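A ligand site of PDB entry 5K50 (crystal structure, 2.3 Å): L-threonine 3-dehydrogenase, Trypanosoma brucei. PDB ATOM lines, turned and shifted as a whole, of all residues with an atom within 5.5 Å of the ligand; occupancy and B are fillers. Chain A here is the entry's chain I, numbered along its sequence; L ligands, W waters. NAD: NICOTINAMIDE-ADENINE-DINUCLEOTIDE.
SD of Met 79 lies close to O2N of the ligand (3.3 Å).
Gly 7 touches the ligand.
C of Leu 9 touches O3B of the ligand (3.6 Å).
CG2 of Val 35 touches O2B of the ligand, at 3.8 Å.
O of Leu 52 touches C2A of the ligand (3.3 Å).
CB of Pro 76 touches C4A of the ligand (3.7 Å).
CB of Ala 77 touches O3D of the ligand, 3.5 Å away.
Ile 93 touches the ligand.
Pro 115 touches the ligand.
O of Ser 116 touches C6N of the ligand, at 3.5 Å.
Thr 117 touches the ligand (CB to C5N, 3.8 Å).
CB of Leu 169 touches C5N of the ligand, at 3.4 Å.
Pro 170 touches the ligand.
CA of Gly 171 touches O7N of the ligand, 3.9 Å away.
Gly 180 touches the ligand.
Thr 184 touches the ligand.
Hydrophobic or aromatic side chains that line the ligand: Leu 9, Ile 12, Val 34, Val 35, Pro 76, Ala 77, Met 79, Ile 93, Pro 115, Tyr 142, Leu 169 and Ile 172.
Within 4 Å of the ligand: Gly 7, Leu 9, Gly 10, Gln 11, Ile 12, Asp 33, Val 34, Val 35, Leu 52, Asp 53, Cys 54, Leu 75, Pro 76, Ala 77, Met 79, Ile 93, Pro 115, Ser 116, Thr 117, Tyr 142, Lys 146, Leu 169, Pro 170, Gly 171, Ile 172, Gly 180 and Thr 184.
Along chain A the residues within 4 Å of the ligand span positions 7 to 184.
OD1 of Asp 33 lies within hydrogen-bond range of O2B of the ligand, 2.4 Å away.
An oxygen (O2D) of the ligand is in hydrogen-bond range of the side-chain hydroxyl (OH) of Tyr 142 (2.4 Å).
O of Leu 75 sits close to O3D of the ligand, at 3.0 Å.
OD1 of Asp 53 sits at hydrogen-bond distance from N6A of the ligand (2.9 Å).
The side-chain amino group (NZ) of Lys 146 lies within hydrogen-bond range of an oxygen (O3D) of the ligand, 2.9 Å away.
The backbone NH (N) of Ile 12 sits at hydrogen-bond distance from an oxygen (O1N) of the ligand, 3.0 Å away.
N of Cys 54 lies within hydrogen-bond range of N1A of the ligand (3.1 Å).
O7N of the ligand lies within hydrogen-bond range of N of Ile 172 (3.1 Å).
O1A of the ligand is in hydrogen-bond range of N of Gln 11 (3.1 Å).
A nitrogen (N7N) of the ligand lies within hydrogen-bond range of the side-chain amide oxygen (OE1) of Gln 11 (3.3 Å).
The backbone NH (N) of Val 34 sits at hydrogen-bond distance from a nitrogen (N3A) of the ligand (3.2 Å).
The backbone NH (N) of Gly 10 sits at hydrogen-bond distance from an oxygen (O3B) of the ligand (3.4 Å).
The backbone NH of Leu 52 is in hydrogen-bond range of the backbone carbonyl oxygen of Asp 33, 2.8 Å away.
The side-chain carboxylate of Asp 33 sits at hydrogen-bond distance from the backbone NH of Leu 9, at 3.2 Å.
The backbone NH (N) of Leu 75 is in hydrogen-bond range of the backbone carbonyl oxygen (O) of Thr 6, 3.1 Å away.
OD1 of Asp 53 lies within hydrogen-bond range of N of Leu 55, at 3.0 Å.
The side-chain amino group (NZ) of Lys 146 sits at hydrogen-bond distance from the backbone carbonyl oxygen (O) of Pro 115.
O of Leu 52 lies within hydrogen-bond range of N of Val 34 (3.4 Å).
The backbone NH (N) of Leu 169 lies within hydrogen-bond range of the backbone carbonyl oxygen (O) of Ser 116.
The backbone carbonyl oxygen of Ile 93 lies within hydrogen-bond range of the side-chain hydroxyl of Thr 97, at 2.4 Å.
Water W1 lies within hydrogen-bond range of an oxygen (O1N) of the ligand, the backbone carbonyl oxygen (O) of Gly 7, the backbone NH (N) of Gly 13 and the backbone NH (N) of Gly 10.
Water W2 lies within hydrogen-bond range of O of Leu 52 (3.0 Å), OG of Ser 32 (3.1 Å) and SG of Cys 54 (3.2 Å).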
ATOM      1  N   THR A   6       2.468   1.868 -34.364  1.00  0.00           N
ATOM      2  CA  THR A   6       2.885   2.911 -33.452  1.00  0.00           C
ATOM      3  C   THR A   6       3.715   2.283 -32.370  1.00  0.00           C
ATOM      4  O   THR A   6       3.510   1.134 -32.029  1.00  0.00           O
ATOM      5  CB  THR A   6       1.676   3.702 -32.863  1.00  0.00           C
ATOM      6  OG1 THR A   6       0.808   2.847 -32.076  1.00  0.00           O
ATOM      7  CG2 THR A   6       0.875   4.344 -33.947  1.00  0.00           C
ATOM      8  N   GLY A   7       4.635   3.037 -31.801  1.00  0.00           N
ATOM      9  CA  GLY A   7       5.593   2.477 -30.840  1.00  0.00           C
ATOM     10  C   GLY A   7       6.538   1.454 -31.472  1.00  0.00           C
ATOM     11  O   GLY A   7       7.058   0.550 -30.806  1.00  0.00           O
ATOM     12  N   ALA A   8       6.797   1.620 -32.780  1.00  0.00           N
ATOM     13  CA  ALA A   8       7.460   0.595 -33.571  1.00  0.00           C
ATOM     14  C   ALA A   8       8.898   0.278 -33.187  1.00  0.00           C
ATOM     15  O   ALA A   8       9.376  -0.837 -33.402  1.00  0.00           O
ATOM     16  CB  ALA A   8       7.400   0.976 -35.047  1.00  0.00           C
ATOM     17  N   LEU A   9       9.625   1.247 -32.633  1.00  0.00           N
ATOM     18  CA  LEU A   9      11.067   1.020 -32.413  1.00  0.00           C
ATOM     19  C   LEU A   9      11.385   0.148 -31.217  1.00  0.00           C
ATOM     20  O   LEU A   9      12.531  -0.030 -30.885  1.00  0.00           O
ATOM     21  CB  LEU A   9      11.799   2.349 -32.274  1.00  0.00           C
ATOM     22  CG  LEU A   9      11.811   3.241 -33.513  1.00  0.00           C
ATOM     23  CD1 LEU A   9      12.744   4.425 -33.261  1.00  0.00           C
ATOM     24  CD2 LEU A   9      12.222   2.517 -34.796  1.00  0.00           C
ATOM     25  N   GLY A  10      10.383  -0.427 -30.566  1.00  0.00           N
ATOM     26  CA  GLY A  10      10.629  -1.223 -29.367  1.00  0.00           C
ATOM     27  C   GLY A  10      10.803  -2.682 -29.650  1.00  0.00           C
ATOM     28  O   GLY A  10      10.770  -3.128 -30.799  1.00  0.00           O
ATOM     29  N   GLN A  11      10.992  -3.453 -28.611  1.00  0.00           N
ATOM     30  CA  GLN A  11      11.175  -4.918 -28.743  1.00  0.00           C
ATOM     31  C   GLN A  11      10.194  -5.592 -29.722  1.00  0.00           C
ATOM     32  O   GLN A  11      10.590  -6.219 -30.713  1.00  0.00           O
ATOM     33  CB  GLN A  11      11.013  -5.560 -27.380  1.00  0.00           C
ATOM     34  CG  GLN A  11      11.491  -6.996 -27.375  1.00  0.00           C
ATOM     35  CD  GLN A  11      11.219  -7.642 -26.052  1.00  0.00           C
ATOM     36  OE1 GLN A  11      10.900  -6.955 -25.090  1.00  0.00           O
ATOM     37  NE2 GLN A  11      11.314  -8.978 -25.995  1.00  0.00           N
ATOM     38  N   ILE A  12       8.912  -5.398 -29.468  1.00  0.00           N
ATOM     39  CA  ILE A  12       7.874  -5.999 -30.307  1.00  0.00           C
ATOM     40  C   ILE A  12       7.865  -5.368 -31.690  1.00  0.00           C
ATOM     41  O   ILE A  12       7.926  -6.058 -32.700  1.00  0.00           O
ATOM     42  CB  ILE A  12       6.462  -5.830 -29.692  1.00  0.00           C
ATOM     43  CG1 ILE A  12       6.360  -6.413 -28.265  1.00  0.00           C
ATOM     44  CG2 ILE A  12       5.393  -6.440 -30.584  1.00  0.00           C
ATOM     45  CD1 ILE A  12       6.714  -7.887 -28.093  1.00  0.00           C
ATOM     46  N   GLY A  13       7.756  -4.049 -31.716  1.00  0.00           N
ATOM     47  CA  GLY A  13       7.599  -3.336 -32.965  1.00  0.00           C
ATOM     48  C   GLY A  13       8.695  -3.669 -33.968  1.00  0.00           C
ATOM     49  O   GLY A  13       8.420  -3.903 -35.137  1.00  0.00           O
ATOM     50  N   SER A  32       6.242   4.115 -36.989  1.00  0.00           N
ATOM     51  CA  SER A  32       6.471   5.367 -36.307  1.00  0.00           C
ATOM     52  C   SER A  32       6.708   5.201 -34.843  1.00  0.00           C
ATOM     53  O   SER A  32       6.235   4.261 -34.255  1.00  0.00           O
ATOM     54  CB  SER A  32       5.224   6.296 -36.505  1.00  0.00           C
ATOM     55  OG  SER A  32       4.104   5.923 -35.684  1.00  0.00           O
ATOM     56  N   ASP A  33       7.407   6.147 -34.242  1.00  0.00           N
ATOM     57  CA  ASP A  33       7.743   6.094 -32.836  1.00  0.00           C
ATOM     58  C   ASP A  33       8.094   7.517 -32.343  1.00  0.00           C
ATOM     59  O   ASP A  33       8.376   8.429 -33.155  1.00  0.00           O
ATOM     60  CB  ASP A  33       8.898   5.104 -32.670  1.00  0.00           C
ATOM     61  CG  ASP A  33       9.262   4.855 -31.224  1.00  0.00           C
ATOM     62  OD1 ASP A  33       9.821   5.764 -30.603  1.00  0.00           O
ATOM     63  OD2 ASP A  33       9.032   3.743 -30.680  1.00  0.00           O
ATOM     64  N   VAL A  34       8.068   7.722 -31.019  1.00  0.00           N
ATOM     65  CA  VAL A  34       8.341   9.074 -30.483  1.00  0.00           C
ATOM     66  C   VAL A  34       9.777   9.513 -30.751  1.00  0.00           C
ATOM     67  O   VAL A  34      10.035  10.657 -31.085  1.00  0.00           O
ATOM     68  CB  VAL A  34       7.999   9.220 -28.991  1.00  0.00           C
ATOM     69  CG1 VAL A  34       8.692   8.175 -28.138  1.00  0.00           C
ATOM     70  CG2 VAL A  34       8.336  10.635 -28.513  1.00  0.00           C
ATOM     71  N   VAL A  35      10.712   8.587 -30.607  1.00  0.00           N
ATOM     72  CA  VAL A  35      12.099   8.857 -30.957  1.00  0.00           C
ATOM     73  C   VAL A  35      12.409   8.506 -32.420  1.00  0.00           C
ATOM     74  O   VAL A  35      11.590   7.938 -33.153  1.00  0.00           O
ATOM     75  CB  VAL A  35      13.074   8.124 -30.012  1.00  0.00           C
ATOM     76  CG1 VAL A  35      12.927   8.658 -28.603  1.00  0.00           C
ATOM     77  CG2 VAL A  35      12.866   6.615 -30.023  1.00  0.00           C
ATOM     78  N   LEU A  52       6.846  10.459 -34.326  1.00  0.00           N
ATOM     79  CA  LEU A  52       5.434  10.772 -33.995  1.00  0.00           C
ATOM     80  C   LEU A  52       5.155  10.507 -32.538  1.00  0.00           C
ATOM     81  O   LEU A  52       5.304   9.383 -32.067  1.00  0.00           O
ATOM     82  CB  LEU A  52       4.453   9.921 -34.811  1.00  0.00           C
ATOM     83  CG  LEU A  52       2.984  10.011 -34.364  1.00  0.00           C
ATOM     84  CD1 LEU A  52       2.410  11.392 -34.680  1.00  0.00           C
ATOM     85  CD2 LEU A  52       2.134   8.927 -35.001  1.00  0.00           C
ATOM     86  N   ASP A  53       4.740  11.541 -31.827  1.00  0.00           N
ATOM     87  CA  ASP A  53       4.345  11.388 -30.459  1.00  0.00           C
ATOM     88  C   ASP A  53       2.845  11.139 -30.488  1.00  0.00           C
ATOM     89  O   ASP A  53       2.082  11.991 -30.947  1.00  0.00           O
ATOM     90  CB  ASP A  53       4.670  12.631 -29.676  1.00  0.00           C
ATOM     91  CG  ASP A  53       4.343  12.509 -28.229  1.00  0.00           C
ATOM     92  OD1 ASP A  53       3.795  11.461 -27.796  1.00  0.00           O
ATOM     93  OD2 ASP A  53       4.634  13.492 -27.510  1.00  0.00           O
ATOM     94  N   CYS A  54       2.438   9.952 -30.021  1.00  0.00           N
ATOM     95  CA  CYS A  54       1.038   9.582 -29.954  1.00  0.00           C
ATOM     96  C   CYS A  54       0.195  10.505 -29.005  1.00  0.00           C
ATOM     97  O   CYS A  54      -1.038  10.609 -29.152  1.00  0.00           O
ATOM     98  CB  CYS A  54       0.950   8.083 -29.648  1.00  0.00           C
ATOM     99  SG  CYS A  54       1.461   7.057 -31.092  1.00  0.00           S
ATOM    100  N   LEU A  55       0.862  11.247 -28.096  1.00  0.00           N
ATOM    101  CA  LEU A  55       0.168  12.248 -27.268  1.00  0.00           C
ATOM    102  C   LEU A  55      -0.179  13.561 -28.015  1.00  0.00           C
ATOM    103  O   LEU A  55      -1.090  14.277 -27.619  1.00  0.00           O
ATOM    104  CB  LEU A  55       0.938  12.523 -25.983  1.00  0.00           C
ATOM    105  CG  LEU A  55       0.803  11.367 -24.963  1.00  0.00           C
ATOM    106  CD1 LEU A  55       1.752  11.523 -23.779  1.00  0.00           C
ATOM    107  CD2 LEU A  55      -0.620  11.194 -24.453  1.00  0.00           C
ATOM    108  N   HIS A  74      -1.170  -0.666 -32.346  1.00  0.00           N
ATOM    109  CA  HIS A  74      -0.857   0.372 -31.379  1.00  0.00           C
ATOM    110  C   HIS A  74      -0.062  -0.105 -30.183  1.00  0.00           C
ATOM    111  O   HIS A  74      -0.627  -0.504 -29.206  1.00  0.00           O
ATOM    112  CB  HIS A  74      -2.126   1.092 -30.871  1.00  0.00           C
ATOM    113  CG  HIS A  74      -1.829   2.200 -29.916  1.00  0.00           C
ATOM    114  ND1 HIS A  74      -1.347   3.418 -30.339  1.00  0.00           N
ATOM    115  CD2 HIS A  74      -1.872   2.262 -28.571  1.00  0.00           C
ATOM    116  CE1 HIS A  74      -1.138   4.195 -29.295  1.00  0.00           C
ATOM    117  NE2 HIS A  74      -1.459   3.514 -28.206  1.00  0.00           N
ATOM    118  N   LEU A  75       1.250  -0.005 -30.230  1.00  0.00           N
ATOM    119  CA  LEU A  75       2.118  -0.652 -29.219  1.00  0.00           C
ATOM    120  C   LEU A  75       2.681   0.182 -28.064  1.00  0.00           C
ATOM    121  O   LEU A  75       3.209  -0.422 -27.130  1.00  0.00           O
ATOM    122  CB  LEU A  75       3.301  -1.308 -29.910  1.00  0.00           C
ATOM    123  CG  LEU A  75       2.976  -2.052 -31.184  1.00  0.00           C
ATOM    124  CD1 LEU A  75       4.333  -2.475 -31.794  1.00  0.00           C
ATOM    125  CD2 LEU A  75       2.125  -3.261 -30.918  1.00  0.00           C
ATOM    126  N   PRO A  76       2.578   1.539 -28.090  1.00  0.00           N
ATOM    127  CA  PRO A  76       3.266   2.209 -26.965  1.00  0.00           C
ATOM    128  C   PRO A  76       2.559   2.074 -25.612  1.00  0.00           C
ATOM    129  O   PRO A  76       1.358   2.241 -25.505  1.00  0.00           O
ATOM    130  CB  PRO A  76       3.340   3.701 -27.394  1.00  0.00           C
ATOM    131  CG  PRO A  76       2.308   3.850 -28.487  1.00  0.00           C
ATOM    132  CD  PRO A  76       1.958   2.502 -29.031  1.00  0.00           C
ATOM    133  N   ALA A  77       3.328   1.773 -24.582  1.00  0.00           N
ATOM    134  CA  ALA A  77       2.880   1.773 -23.224  1.00  0.00           C
ATOM    135  C   ALA A  77       4.146   1.972 -22.388  1.00  0.00           C
ATOM    136  O   ALA A  77       5.248   1.907 -22.942  1.00  0.00           O
ATOM    137  CB  ALA A  77       2.212   0.451 -22.879  1.00  0.00           C
ATOM    138  N   ILE A  78       4.003   2.236 -21.106  1.00  0.00           N
ATOM    139  CA  ILE A  78       5.134   2.146 -20.187  1.00  0.00           C
ATOM    140  C   ILE A  78       4.886   0.866 -19.402  1.00  0.00           C
ATOM    141  O   ILE A  78       3.775   0.675 -18.878  1.00  0.00           O
ATOM    142  CB  ILE A  78       5.189   3.312 -19.204  1.00  0.00           C
ATOM    143  CG1 ILE A  78       5.423   4.671 -19.907  1.00  0.00           C
ATOM    144  CG2 ILE A  78       6.266   3.059 -18.152  1.00  0.00           C
ATOM    145  CD1 ILE A  78       6.612   4.786 -20.857  1.00  0.00           C
ATOM    146  N   MET A  79       5.892  -0.017 -19.324  1.00  0.00           N
ATOM    147  CA  MET A  79       5.659  -1.369 -18.805  1.00  0.00           C
ATOM    148  C   MET A  79       5.868  -1.433 -17.293  1.00  0.00           C
ATOM    149  O   MET A  79       5.934  -0.390 -16.615  1.00  0.00           O
ATOM    150  CB  MET A  79       6.442  -2.425 -19.626  1.00  0.00           C
ATOM    151  CG  MET A  79       5.845  -2.577 -21.039  1.00  0.00           C
ATOM    152  SD  MET A  79       6.792  -3.524 -22.240  1.00  0.00           S
ATOM    153  CE  MET A  79       7.123  -4.886 -21.173  1.00  0.00           C
ATOM    154  N   ILE A  93       0.656   7.942 -21.152  1.00  0.00           N
ATOM    155  CA  ILE A  93       0.873   7.223 -22.387  1.00  0.00           C
ATOM    156  C   ILE A  93      -0.195   6.123 -22.553  1.00  0.00           C
ATOM    157  O   ILE A  93      -0.753   5.998 -23.651  1.00  0.00           O
ATOM    158  CB  ILE A  93       2.271   6.530 -22.457  1.00  0.00           C
ATOM    159  CG1 ILE A  93       3.421   7.461 -22.122  1.00  0.00           C
ATOM    160  CG2 ILE A  93       2.473   5.925 -23.844  1.00  0.00           C
ATOM    161  CD1 ILE A  93       3.864   8.396 -23.227  1.00  0.00           C
ATOM    162  N   THR A  97      -2.865   7.824 -25.128  1.00  0.00           N
ATOM    163  CA  THR A  97      -2.521   7.361 -26.498  1.00  0.00           C
ATOM    164  C   THR A  97      -3.505   6.313 -26.963  1.00  0.00           C
ATOM    165  O   THR A  97      -3.877   6.277 -28.140  1.00  0.00           O
ATOM    166  CB  THR A  97      -1.065   6.802 -26.673  1.00  0.00           C
ATOM    167  OG1 THR A  97      -0.903   5.495 -26.042  1.00  0.00           O
ATOM    168  CG2 THR A  97      -0.030   7.804 -26.138  1.00  0.00           C
ATOM    169  N   PRO A 115      -2.110  -4.582 -27.777  1.00  0.00           N
ATOM    170  CA  PRO A 115      -1.792  -5.627 -26.883  1.00  0.00           C
ATOM    171  C   PRO A 115      -2.176  -5.326 -25.427  1.00  0.00           C
ATOM    172  O   PRO A 115      -1.925  -4.246 -24.914  1.00  0.00           O
ATOM    173  CB  PRO A 115      -0.284  -5.713 -26.988  1.00  0.00           C
ATOM    174  CG  PRO A 115       0.149  -4.298 -27.197  1.00  0.00           C
ATOM    175  CD  PRO A 115      -0.949  -3.737 -28.093  1.00  0.00           C
ATOM    176  N   SER A 116      -2.797  -6.293 -24.798  1.00  0.00           N
ATOM    177  CA  SER A 116      -2.835  -6.356 -23.359  1.00  0.00           C
ATOM    178  C   SER A 116      -1.698  -7.262 -22.895  1.00  0.00           C
ATOM    179  O   SER A 116      -0.715  -7.483 -23.621  1.00  0.00           O
ATOM    180  CB  SER A 116      -4.193  -6.862 -22.905  1.00  0.00           C
ATOM    181  OG  SER A 116      -4.299  -6.781 -21.492  1.00  0.00           O
ATOM    182  N   THR A 117      -1.820  -7.784 -21.693  1.00  0.00           N
ATOM    183  CA  THR A 117      -0.725  -8.469 -21.024  1.00  0.00           C
ATOM    184  C   THR A 117      -1.216  -9.284 -19.816  1.00  0.00           C
ATOM    185  O   THR A 117      -2.264  -8.951 -19.226  1.00  0.00           O
ATOM    186  CB  THR A 117       0.332  -7.467 -20.495  1.00  0.00           C
ATOM    187  OG1 THR A 117       1.174  -8.097 -19.524  1.00  0.00           O
ATOM    188  CG2 THR A 117      -0.313  -6.305 -19.787  1.00  0.00           C
ATOM    189  N   TYR A 142       0.611  -0.274 -14.474  1.00  0.00           N
ATOM    190  CA  TYR A 142       0.640  -0.807 -15.826  1.00  0.00           C
ATOM    191  C   TYR A 142      -0.556  -1.654 -16.091  1.00  0.00           C
ATOM    192  O   TYR A 142      -1.329  -1.367 -17.009  1.00  0.00           O
ATOM    193  CB  TYR A 142       1.932  -1.608 -15.986  1.00  0.00           C
ATOM    194  CG  TYR A 142       2.142  -2.403 -17.264  1.00  0.00           C
ATOM    195  CD1 TYR A 142       2.040  -1.828 -18.485  1.00  0.00           C
ATOM    196  CD2 TYR A 142       2.505  -3.746 -17.203  1.00  0.00           C
ATOM    197  CE1 TYR A 142       2.269  -2.535 -19.651  1.00  0.00           C
ATOM    198  CE2 TYR A 142       2.704  -4.478 -18.354  1.00  0.00           C
ATOM    199  CZ  TYR A 142       2.597  -3.873 -19.581  1.00  0.00           C
ATOM    200  OH  TYR A 142       2.841  -4.586 -20.772  1.00  0.00           O
ATOM    201  N   LYS A 146      -4.125  -1.345 -18.381  1.00  0.00           N
ATOM    202  CA  LYS A 146      -4.271  -2.251 -19.477  1.00  0.00           C
ATOM    203  C   LYS A 146      -5.637  -2.902 -19.339  1.00  0.00           C
ATOM    204  O   LYS A 146      -6.262  -3.214 -20.359  1.00  0.00           O
ATOM    205  CB  LYS A 146      -3.166  -3.297 -19.517  1.00  0.00           C
ATOM    206  CG  LYS A 146      -1.842  -2.781 -20.039  1.00  0.00           C
ATOM    207  CD  LYS A 146      -1.906  -2.469 -21.519  1.00  0.00           C
ATOM    208  CE  LYS A 146      -0.519  -2.437 -22.133  1.00  0.00           C
ATOM    209  NZ  LYS A 146      -0.667  -2.038 -23.543  1.00  0.00           N
ATOM    210  N   LEU A 169      -0.405 -10.598 -24.135  1.00  0.00           N
ATOM    211  CA  LEU A 169       0.907 -11.171 -24.381  1.00  0.00           C
ATOM    212  C   LEU A 169       1.563 -11.517 -23.056  1.00  0.00           C
ATOM    213  O   LEU A 169       1.413 -10.807 -22.066  1.00  0.00           O
ATOM    214  CB  LEU A 169       1.853 -10.227 -25.138  1.00  0.00           C
ATOM    215  CG  LEU A 169       1.631  -9.974 -26.608  1.00  0.00           C
ATOM    216  CD1 LEU A 169       2.523  -8.789 -27.000  1.00  0.00           C
ATOM    217  CD2 LEU A 169       1.902 -11.219 -27.448  1.00  0.00           C
ATOM    218  N   PRO A 170       2.258 -12.646 -23.034  1.00  0.00           N
ATOM    219  CA  PRO A 170       3.102 -12.994 -21.940  1.00  0.00           C
ATOM    220  C   PRO A 170       4.504 -12.419 -22.134  1.00  0.00           C
ATOM    221  O   PRO A 170       4.772 -11.699 -23.109  1.00  0.00           O
ATOM    222  CB  PRO A 170       3.124 -14.514 -22.008  1.00  0.00           C
ATOM    223  CG  PRO A 170       3.002 -14.829 -23.464  1.00  0.00           C
ATOM    224  CD  PRO A 170       2.154 -13.726 -24.035  1.00  0.00           C
ATOM    225  N   GLY A 171       5.400 -12.744 -21.223  1.00  0.00           N
ATOM    226  CA  GLY A 171       6.824 -12.466 -21.447  1.00  0.00           C
ATOM    227  C   GLY A 171       7.158 -12.859 -22.875  1.00  0.00           C
ATOM    228  O   GLY A 171       6.909 -14.005 -23.264  1.00  0.00           O
ATOM    229  N   ILE A 172       7.652 -11.892 -23.659  1.00  0.00           N
ATOM    230  CA  ILE A 172       8.132 -12.113 -25.024  1.00  0.00           C
ATOM    231  C   ILE A 172       9.662 -12.008 -25.141  1.00  0.00           C
ATOM    232  O   ILE A 172      10.219 -10.958 -24.835  1.00  0.00           O
ATOM    233  CB  ILE A 172       7.610 -11.069 -26.006  1.00  0.00           C
ATOM    234  CG1 ILE A 172       6.086 -10.891 -25.918  1.00  0.00           C
ATOM    235  CG2 ILE A 172       8.048 -11.462 -27.412  1.00  0.00           C
ATOM    236  CD1 ILE A 172       5.286 -12.112 -26.343  1.00  0.00           C
ATOM    237  N   THR A 177      16.272  -6.265 -30.183  1.00  0.00           N
ATOM    238  CA  THR A 177      16.191  -5.070 -29.347  1.00  0.00           C
ATOM    239  C   THR A 177      16.025  -5.453 -27.842  1.00  0.00           C
ATOM    240  O   THR A 177      15.159  -6.278 -27.484  1.00  0.00           O
ATOM    241  CB  THR A 177      15.053  -4.148 -29.879  1.00  0.00           C
ATOM    242  OG1 THR A 177      15.437  -3.563 -31.147  1.00  0.00           O
ATOM    243  CG2 THR A 177      14.724  -3.023 -28.894  1.00  0.00           C
ATOM    244  N   LEU A 178      16.888  -4.875 -26.996  1.00  0.00           N
ATOM    245  CA  LEU A 178      16.816  -5.079 -25.544  1.00  0.00           C
ATOM    246  C   LEU A 178      15.499  -4.473 -25.025  1.00  0.00           C
ATOM    247  O   LEU A 178      15.082  -3.409 -25.495  1.00  0.00           O
ATOM    248  CB  LEU A 178      18.016  -4.447 -24.795  1.00  0.00           C
ATOM    249  CG  LEU A 178      19.406  -5.119 -24.696  1.00  0.00           C
ATOM    250  CD1 LEU A 178      19.326  -6.495 -24.068  1.00  0.00           C
ATOM    251  CD2 LEU A 178      20.104  -5.169 -26.054  1.00  0.00           C
ATOM    252  N   PRO A 179      14.857  -5.114 -24.029  1.00  0.00           N
ATOM    253  CA  PRO A 179      13.488  -4.761 -23.636  1.00  0.00           C
ATOM    254  C   PRO A 179      13.385  -3.407 -22.919  1.00  0.00           C
ATOM    255  O   PRO A 179      14.421  -2.836 -22.534  1.00  0.00           O
ATOM    256  CB  PRO A 179      13.086  -5.904 -22.696  1.00  0.00           C
ATOM    257  CG  PRO A 179      14.373  -6.322 -22.057  1.00  0.00           C
ATOM    258  CD  PRO A 179      15.458  -6.074 -23.072  1.00  0.00           C
ATOM    259  N   GLY A 180      12.149  -2.944 -22.702  1.00  0.00           N
ATOM    260  CA  GLY A 180      11.873  -1.578 -22.235  1.00  0.00           C
ATOM    261  C   GLY A 180      11.393  -1.329 -20.812  1.00  0.00           C
ATOM    262  O   GLY A 180      10.485  -0.516 -20.602  1.00  0.00           O
ATOM    263  N   THR A 184      10.189  -9.180 -17.288  1.00  0.00           N
ATOM    264  CA  THR A 184      10.666 -10.362 -17.993  1.00  0.00           C
ATOM    265  C   THR A 184      12.016 -10.127 -18.657  1.00  0.00           C
ATOM    266  O   THR A 184      12.556 -11.033 -19.299  1.00  0.00           O
ATOM    267  CB  THR A 184       9.643 -10.848 -19.027  1.00  0.00           C
ATOM    268  OG1 THR A 184       9.309  -9.776 -19.902  1.00  0.00           O
ATOM    269  CG2 THR A 184       8.408 -11.323 -18.307  1.00  0.00           C
HETATM  270  PA  NAD L   1       9.109  -1.028 -25.645  1.00  0.00           P
HETATM  271  O1A NAD L   1      10.223  -1.933 -26.058  1.00  0.00           O
HETATM  272  O2A NAD L   1       9.229  -0.300 -24.367  1.00  0.00           O
HETATM  273  O5B NAD L   1       8.708  -0.111 -26.848  1.00  0.00           O
HETATM  274  C5B NAD L   1       7.781   0.941 -26.638  1.00  0.00           C
HETATM  275  C4B NAD L   1       7.984   1.993 -27.697  1.00  0.00           C
HETATM  276  O4B NAD L   1       7.041   3.015 -27.474  1.00  0.00           O
HETATM  277  C3B NAD L   1       9.389   2.654 -27.569  1.00  0.00           C
HETATM  278  O3B NAD L   1      10.013   2.416 -28.813  1.00  0.00           O
HETATM  279  C2B NAD L   1       9.141   4.133 -27.408  1.00  0.00           C
HETATM  280  O2B NAD L   1       9.929   4.935 -28.329  1.00  0.00           O
HETATM  281  C1B NAD L   1       7.699   4.186 -27.929  1.00  0.00           C
HETATM  282  N9A NAD L   1       6.924   5.252 -27.297  1.00  0.00           N
HETATM  283  C8A NAD L   1       6.812   5.547 -25.989  1.00  0.00           C
HETATM  284  N7A NAD L   1       5.979   6.594 -25.872  1.00  0.00           N
HETATM  285  C5A NAD L   1       5.575   6.932 -27.090  1.00  0.00           C
HETATM  286  C6A NAD L   1       4.730   7.922 -27.558  1.00  0.00           C
HETATM  287  N6A NAD L   1       4.145   8.767 -26.704  1.00  0.00           N
HETATM  288  N1A NAD L   1       4.515   8.010 -28.892  1.00  0.00           N
HETATM  289  C2A NAD L   1       5.118   7.132 -29.712  1.00  0.00           C
HETATM  290  N3A NAD L   1       5.935   6.157 -29.293  1.00  0.00           N
HETATM  291  C4A NAD L   1       6.173   6.068 -27.988  1.00  0.00           C
HETATM  292  O3  NAD L   1       7.743  -1.889 -25.574  1.00  0.00           O
HETATM  293  PN  NAD L   1       7.534  -3.440 -26.047  1.00  0.00           P
HETATM  294  O1N NAD L   1       7.820  -3.484 -27.472  1.00  0.00           O
HETATM  295  O2N NAD L   1       8.129  -4.348 -25.101  1.00  0.00           O
HETATM  296  O5D NAD L   1       5.966  -3.611 -25.816  1.00  0.00           O
HETATM  297  C5D NAD L   1       5.118  -2.773 -26.568  1.00  0.00           C
HETATM  298  C4D NAD L   1       3.696  -3.119 -26.360  1.00  0.00           C
HETATM  299  O4D NAD L   1       3.691  -4.555 -26.204  1.00  0.00           O
HETATM  300  C3D NAD L   1       3.167  -2.498 -25.047  1.00  0.00           C
HETATM  301  O3D NAD L   1       1.779  -2.179 -25.177  1.00  0.00           O
HETATM  302  C2D NAD L   1       3.371  -3.594 -24.061  1.00  0.00           C
HETATM  303  O2D NAD L   1       2.455  -3.530 -22.940  1.00  0.00           O
HETATM  304  C1D NAD L   1       3.094  -4.800 -24.966  1.00  0.00           C
HETATM  305  N1N NAD L   1       3.666  -5.975 -24.344  1.00  0.00           N
HETATM  306  C2N NAD L   1       4.994  -6.335 -24.454  1.00  0.00           C
HETATM  307  C3N NAD L   1       5.424  -7.524 -23.817  1.00  0.00           C
HETATM  308  C7N NAD L   1       6.884  -8.013 -23.850  1.00  0.00           C
HETATM  309  O7N NAD L   1       7.358  -8.921 -22.963  1.00  0.00           O
HETATM  310  N7N NAD L   1       7.660  -7.499 -24.760  1.00  0.00           N
HETATM  311  C4N NAD L   1       4.523  -8.278 -23.078  1.00  0.00           C
HETATM  312  C5N NAD L   1       3.182  -7.902 -22.979  1.00  0.00           C
HETATM  313  C6N NAD L   1       2.750  -6.758 -23.615  1.00  0.00           C
HETATM  314  O   HOH W   1       7.521  -2.025 -29.542  1.00  0.00           O
HETATM  315  O   HOH W   2       4.142   6.667 -32.705  1.00  0.00           O
HETATM  316  O   HOH W   3       0.067  -0.416 -26.515  1.00  0.00           O
